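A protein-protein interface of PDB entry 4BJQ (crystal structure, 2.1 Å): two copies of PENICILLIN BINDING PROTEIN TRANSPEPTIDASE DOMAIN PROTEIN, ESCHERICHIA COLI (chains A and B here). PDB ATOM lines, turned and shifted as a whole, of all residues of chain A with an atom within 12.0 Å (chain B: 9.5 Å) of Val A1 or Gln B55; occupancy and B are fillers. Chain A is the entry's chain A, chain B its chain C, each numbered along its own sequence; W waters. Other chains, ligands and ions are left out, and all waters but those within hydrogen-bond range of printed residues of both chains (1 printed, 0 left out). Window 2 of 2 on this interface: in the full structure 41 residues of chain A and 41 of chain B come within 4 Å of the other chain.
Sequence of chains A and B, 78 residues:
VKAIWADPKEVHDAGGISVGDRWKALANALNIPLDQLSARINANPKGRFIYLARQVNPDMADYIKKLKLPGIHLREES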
ATOM      1  N   VAL A   1      10.718  -3.345  27.091  1.00  0.00           N
ATOM      2  CA  VAL A   1      11.157  -2.515  25.927  1.00  0.00           C
ATOM      3  C   VAL A   1      10.553  -3.063  24.617  1.00  0.00           C
ATOM      4  O   VAL A   1      10.642  -4.262  24.334  1.00  0.00           O
ATOM      5  CB  VAL A   1      12.716  -2.358  25.907  1.00  0.00           C
ATOM      6  CG1 VAL A   1      13.294  -2.492  24.514  1.00  0.00           C
ATOM      7  CG2 VAL A   1      13.140  -1.021  26.547  1.00  0.00           C
ATOM      8  N   LYS A   2       9.918  -2.184  23.839  1.00  0.00           N
ATOM      9  CA  LYS A   2       9.122  -2.628  22.686  1.00  0.00           C
ATOM     10  C   LYS A   2       9.631  -2.149  21.320  1.00  0.00           C
ATOM     11  O   LYS A   2      10.305  -1.122  21.214  1.00  0.00           O
ATOM     12  CB  LYS A   2       7.651  -2.211  22.845  1.00  0.00           C
ATOM     13  CG  LYS A   2       6.966  -2.620  24.149  1.00  0.00           C
ATOM     14  CD  LYS A   2       6.554  -4.090  24.187  1.00  0.00           C
ATOM     15  CE  LYS A   2       5.657  -4.386  25.400  1.00  0.00           C
ATOM     16  NZ  LYS A   2       6.252  -3.881  26.691  1.00  0.00           N
ATOM     17  N   ALA A   3       9.298  -2.917  20.286  1.00  0.00           N
ATOM     18  CA  ALA A   3       9.365  -2.450  18.904  1.00  0.00           C
ATOM     19  C   ALA A   3       7.969  -2.025  18.476  1.00  0.00           C
ATOM     20  O   ALA A   3       6.977  -2.677  18.821  1.00  0.00           O
ATOM     21  CB  ALA A   3       9.881  -3.549  17.978  1.00  0.00           C
ATOM     22  N   ILE A   4       7.897  -0.917  17.743  1.00  0.00           N
ATOM     23  CA  ILE A   4       6.653  -0.493  17.123  1.00  0.00           C
ATOM     24  C   ILE A   4       6.712  -0.811  15.636  1.00  0.00           C
ATOM     25  O   ILE A   4       7.699  -0.473  14.953  1.00  0.00           O
ATOM     26  CB  ILE A   4       6.407   1.022  17.288  1.00  0.00           C
ATOM     27  CG1 ILE A   4       6.597   1.472  18.755  1.00  0.00           C
ATOM     28  CG2 ILE A   4       5.033   1.415  16.694  1.00  0.00           C
ATOM     29  CD1 ILE A   4       5.545   0.975  19.727  1.00  0.00           C
ATOM     30  N   TRP A   5       5.653  -1.446  15.140  1.00  0.00           N
ATOM     31  CA  TRP A   5       5.558  -1.753  13.729  1.00  0.00           C
ATOM     32  C   TRP A   5       4.186  -1.470  13.134  1.00  0.00           C
ATOM     33  O   TRP A   5       3.184  -1.451  13.846  1.00  0.00           O
ATOM     34  CB  TRP A   5       6.013  -3.181  13.436  1.00  0.00           C
ATOM     35  CG  TRP A   5       5.249  -4.318  14.082  1.00  0.00           C
ATOM     36  CD1 TRP A   5       5.392  -4.788  15.366  1.00  0.00           C
ATOM     37  CD2 TRP A   5       4.305  -5.191  13.443  1.00  0.00           C
ATOM     38  NE1 TRP A   5       4.586  -5.894  15.561  1.00  0.00           N
ATOM     39  CE2 TRP A   5       3.901  -6.152  14.402  1.00  0.00           C
ATOM     40  CE3 TRP A   5       3.750  -5.248  12.152  1.00  0.00           C
ATOM     41  CZ2 TRP A   5       2.956  -7.146  14.116  1.00  0.00           C
ATOM     42  CZ3 TRP A   5       2.819  -6.260  11.859  1.00  0.00           C
ATOM     43  CH2 TRP A   5       2.434  -7.189  12.838  1.00  0.00           C
ATOM     44  N   TYR B  51       8.987  -1.785  10.331  1.00  0.00           N
ATOM     45  CA  TYR B  51       9.356  -1.239  11.642  1.00  0.00           C
ATOM     46  C   TYR B  51       9.142   0.271  11.668  1.00  0.00           C
ATOM     47  O   TYR B  51       9.460   0.966  10.699  1.00  0.00           O
ATOM     48  CB  TYR B  51      10.812  -1.571  12.001  1.00  0.00           C
ATOM     49  CG  TYR B  51      11.029  -2.959  12.598  1.00  0.00           C
ATOM     50  CD1 TYR B  51      10.459  -3.311  13.831  1.00  0.00           C
ATOM     51  CD2 TYR B  51      11.828  -3.902  11.948  1.00  0.00           C
ATOM     52  CE1 TYR B  51      10.664  -4.576  14.390  1.00  0.00           C
ATOM     53  CE2 TYR B  51      12.051  -5.168  12.507  1.00  0.00           C
ATOM     54  CZ  TYR B  51      11.457  -5.500  13.723  1.00  0.00           C
ATOM     55  OH  TYR B  51      11.662  -6.753  14.276  1.00  0.00           O
ATOM     56  N   LEU B  52       8.601   0.775  12.775  1.00  0.00           N
ATOM     57  CA  LEU B  52       8.466   2.219  12.981  1.00  0.00           C
ATOM     58  C   LEU B  52       9.504   2.747  13.999  1.00  0.00           C
ATOM     59  O   LEU B  52      10.075   3.827  13.822  1.00  0.00           O
ATOM     60  CB  LEU B  52       7.049   2.581  13.434  1.00  0.00           C
ATOM     61  CG  LEU B  52       5.894   2.393  12.446  1.00  0.00           C
ATOM     62  CD1 LEU B  52       4.613   3.041  13.003  1.00  0.00           C
ATOM     63  CD2 LEU B  52       6.201   2.959  11.048  1.00  0.00           C
ATOM     64  N   ALA B  53       9.732   1.986  15.063  1.00  0.00           N
ATOM     65  CA  ALA B  53      10.701   2.359  16.076  1.00  0.00           C
ATOM     66  C   ALA B  53      11.165   1.132  16.821  1.00  0.00           C
ATOM     67  O   ALA B  53      10.411   0.175  16.971  1.00  0.00           O
ATOM     68  CB  ALA B  53      10.096   3.383  17.069  1.00  0.00           C
ATOM     69  N   ARG B  54      12.398   1.197  17.318  1.00  0.00           N
ATOM     70  CA  ARG B  54      13.000   0.110  18.070  1.00  0.00           C
ATOM     71  C   ARG B  54      13.359   0.556  19.485  1.00  0.00           C
ATOM     72  O   ARG B  54      13.572   1.750  19.736  1.00  0.00           O
ATOM     73  CB  ARG B  54      14.255  -0.403  17.351  1.00  0.00           C
ATOM     74  CG  ARG B  54      14.020  -0.804  15.910  1.00  0.00           C
ATOM     75  CD  ARG B  54      13.068  -1.991  15.824  1.00  0.00           C
ATOM     76  NE  ARG B  54      13.617  -3.188  16.462  1.00  0.00           N
ATOM     77  CZ  ARG B  54      14.490  -4.019  15.891  1.00  0.00           C
ATOM     78  NH1 ARG B  54      14.924  -3.789  14.657  1.00  0.00           N
ATOM     79  NH2 ARG B  54      14.929  -5.089  16.554  1.00  0.00           N
ATOM     80  N   GLN B  55      13.382  -0.414  20.401  1.00  0.00           N
ATOM     81  CA  GLN B  55      13.863  -0.237  21.784  1.00  0.00           C
ATOM     82  C   GLN B  55      13.151   0.898  22.525  1.00  0.00           C
ATOM     83  O   GLN B  55      13.772   1.649  23.297  1.00  0.00           O
ATOM     84  CB  GLN B  55      15.397  -0.074  21.831  1.00  0.00           C
ATOM     85  CG  GLN B  55      16.204  -1.095  20.984  1.00  0.00           C
ATOM     86  CD  GLN B  55      16.055  -2.547  21.449  1.00  0.00           C
ATOM     87  OE1 GLN B  55      15.785  -2.817  22.622  1.00  0.00           O
ATOM     88  NE2 GLN B  55      16.250  -3.485  20.529  1.00  0.00           N
ATOM     89  N   VAL B  56      11.839   0.991  22.285  1.00  0.00           N
ATOM     90  CA  VAL B  56      10.986   2.059  22.795  1.00  0.00           C
ATOM     91  C   VAL B  56      10.674   1.858  24.272  1.00  0.00           C
ATOM     92  O   VAL B  56      10.254   0.774  24.686  1.00  0.00           O
ATOM     93  CB  VAL B  56       9.648   2.128  22.019  1.00  0.00           C
ATOM     94  CG1 VAL B  56       8.826   3.327  22.465  1.00  0.00           C
ATOM     95  CG2 VAL B  56       9.898   2.200  20.527  1.00  0.00           C
ATOM     96  N   ASN B  57      10.857   2.921  25.052  1.00  0.00           N
ATOM     97  CA  ASN B  57      10.523   2.919  26.477  1.00  0.00           C
ATOM     98  C   ASN B  57       9.076   2.447  26.751  1.00  0.00           C
ATOM     99  O   ASN B  57       8.185   2.700  25.947  1.00  0.00           O
ATOM    100  CB  ASN B  57      10.799   4.306  27.093  1.00  0.00           C
ATOM    101  CG  ASN B  57      12.305   4.599  27.255  1.00  0.00           C
ATOM    102  OD1 ASN B  57      13.165   3.834  26.800  1.00  0.00           O
ATOM    103  ND2 ASN B  57      12.622   5.710  27.911  1.00  0.00           N
ATOM    104  N   PRO B  58       8.856   1.726  27.872  1.00  0.00           N
ATOM    105  CA  PRO B  58       7.543   1.200  28.273  1.00  0.00           C
ATOM    106  C   PRO B  58       6.385   2.200  28.224  1.00  0.00           C
ATOM    107  O   PRO B  58       5.295   1.844  27.772  1.00  0.00           O
ATOM    108  CB  PRO B  58       7.781   0.746  29.716  1.00  0.00           C
ATOM    109  CG  PRO B  58       9.188   0.312  29.720  1.00  0.00           C
ATOM    110  CD  PRO B  58       9.925   1.222  28.755  1.00  0.00           C
ATOM    111  N   ASP B  59       6.618   3.432  28.672  1.00  0.00           N
ATOM    112  CA  ASP B  59       5.550   4.444  28.733  1.00  0.00           C
ATOM    113  C   ASP B  59       5.189   4.993  27.357  1.00  0.00           C
ATOM    114  O   ASP B  59       4.013   5.185  27.042  1.00  0.00           O
ATOM    115  CB  ASP B  59       5.941   5.592  29.666  1.00  0.00           C
ATOM    116  CG  ASP B  59       6.087   5.148  31.112  1.00  0.00           C
ATOM    117  OD1 ASP B  59       6.569   4.020  31.350  1.00  0.00           O
ATOM    118  OD2 ASP B  59       5.729   5.932  32.011  1.00  0.00           O
ATOM    119  N   MET B  60       6.213   5.245  26.547  1.00  0.00           N
ATOM    120  CA  MET B  60       6.024   5.732  25.192  1.00  0.00           C
ATOM    121  C   MET B  60       5.255   4.671  24.398  1.00  0.00           C
ATOM    122  O   MET B  60       4.316   4.995  23.661  1.00  0.00           O
ATOM    123  CB  MET B  60       7.379   6.064  24.551  1.00  0.00           C
ATOM    124  CG  MET B  60       8.209   7.116  25.333  1.00  0.00           C
ATOM    125  SD  MET B  60       9.937   7.331  24.787  1.00  0.00           S
ATOM    126  CE  MET B  60       9.721   7.937  23.102  1.00  0.00           C
ATOM    127  N   ALA B  61       5.629   3.406  24.594  1.00  0.00           N
ATOM    128  CA  ALA B  61       4.968   2.277  23.938  1.00  0.00           C
ATOM    129  C   ALA B  61       3.491   2.171  24.329  1.00  0.00           C
ATOM    130  O   ALA B  61       2.630   1.928  23.476  1.00  0.00           O
ATOM    131  CB  ALA B  61       5.703   0.971  24.233  1.00  0.00           C
ATOM    132  N   ASP B  62       3.205   2.366  25.615  1.00  0.00           N
ATOM    133  CA  ASP B  62       1.828   2.346  26.114  1.00  0.00           C
ATOM    134  C   ASP B  62       0.982   3.514  25.573  1.00  0.00           C
ATOM    135  O   ASP B  62      -0.188   3.337  25.237  1.00  0.00           O
ATOM    136  CB  ASP B  62       1.800   2.293  27.647  1.00  0.00           C
ATOM    137  CG  ASP B  62       0.390   2.163  28.196  1.00  0.00           C
ATOM    138  OD1 ASP B  62      -0.330   1.211  27.813  1.00  0.00           O
ATOM    139  OD2 ASP B  62      -0.014   3.027  28.998  1.00  0.00           O
ATOM    140  N   LEU B  74       2.703  -3.559  18.708  1.00  0.00           N
ATOM    141  CA  LEU B  74       3.859  -3.605  19.589  1.00  0.00           C
ATOM    142  C   LEU B  74       4.356  -5.047  19.685  1.00  0.00           C
ATOM    143  O   LEU B  74       3.561  -5.989  19.682  1.00  0.00           O
ATOM    144  CB  LEU B  74       3.490  -3.105  20.991  1.00  0.00           C
ATOM    145  CG  LEU B  74       3.321  -1.608  21.273  1.00  0.00           C
ATOM    146  CD1 LEU B  74       2.201  -0.963  20.475  1.00  0.00           C
ATOM    147  CD2 LEU B  74       3.064  -1.416  22.760  1.00  0.00           C
ATOM    148  N   ARG B  75       5.668  -5.209  19.747  1.00  0.00           N
ATOM    149  CA  ARG B  75       6.273  -6.500  20.027  1.00  0.00           C
ATOM    150  C   ARG B  75       7.430  -6.265  20.990  1.00  0.00           C
ATOM    151  O   ARG B  75       8.060  -5.203  20.951  1.00  0.00           O
ATOM    152  CB  ARG B  75       6.720  -7.205  18.730  1.00  0.00           C
ATOM    153  CG  ARG B  75       8.093  -6.808  18.192  1.00  0.00           C
ATOM    154  CD  ARG B  75       8.590  -7.779  17.127  1.00  0.00           C
ATOM    155  NE  ARG B  75       8.862  -9.112  17.660  1.00  0.00           N
ATOM    156  CZ  ARG B  75      10.057  -9.701  17.665  1.00  0.00           C
ATOM    157  NH1 ARG B  75      11.123  -9.085  17.154  1.00  0.00           N
ATOM    158  NH2 ARG B  75      10.187 -10.921  18.172  1.00  0.00           N
ATOM    159  N   GLU B  76       7.690  -7.229  21.873  1.00  0.00           N
ATOM    160  CA  GLU B  76       8.766  -7.073  22.852  1.00  0.00           C
ATOM    161  C   GLU B  76      10.105  -7.418  22.201  1.00  0.00           C
ATOM    162  O   GLU B  76      10.221  -8.426  21.511  1.00  0.00           O
ATOM    163  CB  GLU B  76       8.512  -7.925  24.107  1.00  0.00           C
ATOM    164  CG  GLU B  76       8.967  -7.244  25.417  1.00  0.00           C
ATOM    165  CD  GLU B  76       9.074  -8.206  26.598  1.00  0.00           C
ATOM    166  OE1 GLU B  76       8.022  -8.696  27.075  1.00  0.00           O
ATOM    167  OE2 GLU B  76      10.211  -8.465  27.063  1.00  0.00           O
ATOM    168  N   GLU B  77      11.104  -6.562  22.409  1.00  0.00           N
ATOM    169  CA  GLU B  77      12.468  -6.793  21.912  1.00  0.00           C
ATOM    170  C   GLU B  77      13.201  -7.885  22.726  1.00  0.00           C
ATOM    171  O   GLU B  77      12.668  -8.401  23.715  1.00  0.00           O
ATOM    172  CB  GLU B  77      13.277  -5.486  21.971  1.00  0.00           C
ATOM    173  CG  GLU B  77      12.621  -4.264  21.312  1.00  0.00           C
ATOM    174  CD  GLU B  77      12.982  -4.088  19.840  1.00  0.00           C
ATOM    175  OE1 GLU B  77      13.190  -5.099  19.138  1.00  0.00           O
ATOM    176  OE2 GLU B  77      13.049  -2.929  19.381  1.00  0.00           O
ATOM    177  N   SER B  78      14.410  -8.245  22.291  1.00  0.00           N
ATOM    178  CA  SER B  78      15.392  -8.945  23.146  1.00  0.00           C
ATOM    179  C   SER B  78      16.761  -9.008  22.474  1.00  0.00           C
ATOM    180  O   SER B  78      17.477  -8.006  22.425  1.00  0.00           O
ATOM    181  CB  SER B  78      14.929 -10.352  23.561  1.00  0.00           C
ATOM    182  OG  SER B  78      15.511 -11.357  22.750  1.00  0.00           O
HETATM  183  O   HOH W   1       6.898  -6.251  28.799  1.00  0.00           O
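The backbone carbonyl oxygen (O) of Lys A2 is in hydrogen-bond range of the backbone NH (N) of Gln B55 (3.3 Å).
N of Glu B77 is in hydrogen-bond range of O of Val A1 (3.0 Å).
The backbone NH (N) of Leu B52 lies within hydrogen-bond range of the backbone carbonyl oxygen (O) of Ile A4, 2.7 Å away.
O of Ala B53 lies within hydrogen-bond range of N of Ile A4, at 2.8 Å.
The backbone NH of Ala A3 lies within hydrogen-bond range of the backbone carbonyl oxygen of Arg B75 (2.7 Å).
The backbone NH (N) of Val B56 lies within hydrogen-bond range of the backbone carbonyl oxygen (O) of Lys A2 (2.8 Å).
The backbone NH (N) of Gln B55 sits at hydrogen-bond distance from the side-chain carboxylate (OE2) of Glu B77, at 2.7 Å.
The guanidinium group (NE) of Arg B54 lies within salt-bridge range of the side-chain carboxylate (OE2) of Glu B77 (3.0 Å).
Val A1 touches Gln B55.
CA of Val A1 touches O of Val B56 (3.6 Å).
Lys A2 touches Arg B54 (O to C, 3.9 Å).
Lys A2 touches Glu B76 (CD to CA, 3.9 Å).
Glu B77 touches Lys A2.
Tyr B51 touches Ala A3.
Ala A3 touches Glu B77.
Ile A4 touches Tyr B51 (O to C, 3.7 Å).
CG1 of Ile A4 touches CG2 of Val B56 (3.8 Å).
CG of Leu B74 touches CD1 of Ile A4, at 3.7 Å.
Val A1 touches just these residues of chain B: Gln B55, Val B56, Glu B76 and Glu B77.
Of chain A, only Lys A2 comes within 4 Å of Arg B54.
No residue of chain A comes within 4 Å of Asn B57.
No residue of chain A comes within 4 Å of Pro B58.
Glu B77 touches just these residues of chain A: Val A1, Lys A2 and Ala A3.
Of the printed residues of chain A, Leu B74 touches Ala A3 and Ile A4.
Printed residues of chain A within 4 Å of Ala B61: Lys A2 (3.8 Å).
Of the printed residues of chain A, Tyr B51 touches Ala A3 (3.8 Å) and Ile A4 (3.7 Å).
Of the printed residues of chain A, Arg B75 touches Lys A2 and Ala A3.
Printed residues of chain B within 4 Å of Ile A4: Tyr B51 (3.7 Å), Leu B52 (2.7 Å), Ala B53 (2.8 Å), Val B56 (3.8 Å) and Leu B74 (3.7 Å).
The nearest printed residue of chain B that does not touch Ala A3 is Arg B54 (4.05 Å).
Of the 5 printed residues of chain A, 4 touch a printed residue of chain B.
Hydrophobic or aromatic side chains of chain A that line the printed part of chain B: Val A1, Ala A3 and Ile A4.
Hydrophobic or aromatic side chains of chain B within 4 Å of the printed part of chain A: Tyr B51, Leu B52, Val B56, Ala B61 and Leu B74.
Among the printed residues, 21 pairs touch across the chains.
Among the printed residues, no Asp or Glu carboxylate lies within 4 Å of a Lys or Arg side-chain nitrogen of the other chain.
No position is printed for both chains.
Of the 21 pairs that touch across the chains among the printed residues, none has its exchanged pair printed and touching as well.
Water W1 bridges the side-chain carboxylate (OE1) of Glu B76 (3.2 Å) and the side-chain amino group (NZ) of Lys A2 (3.2 Å).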
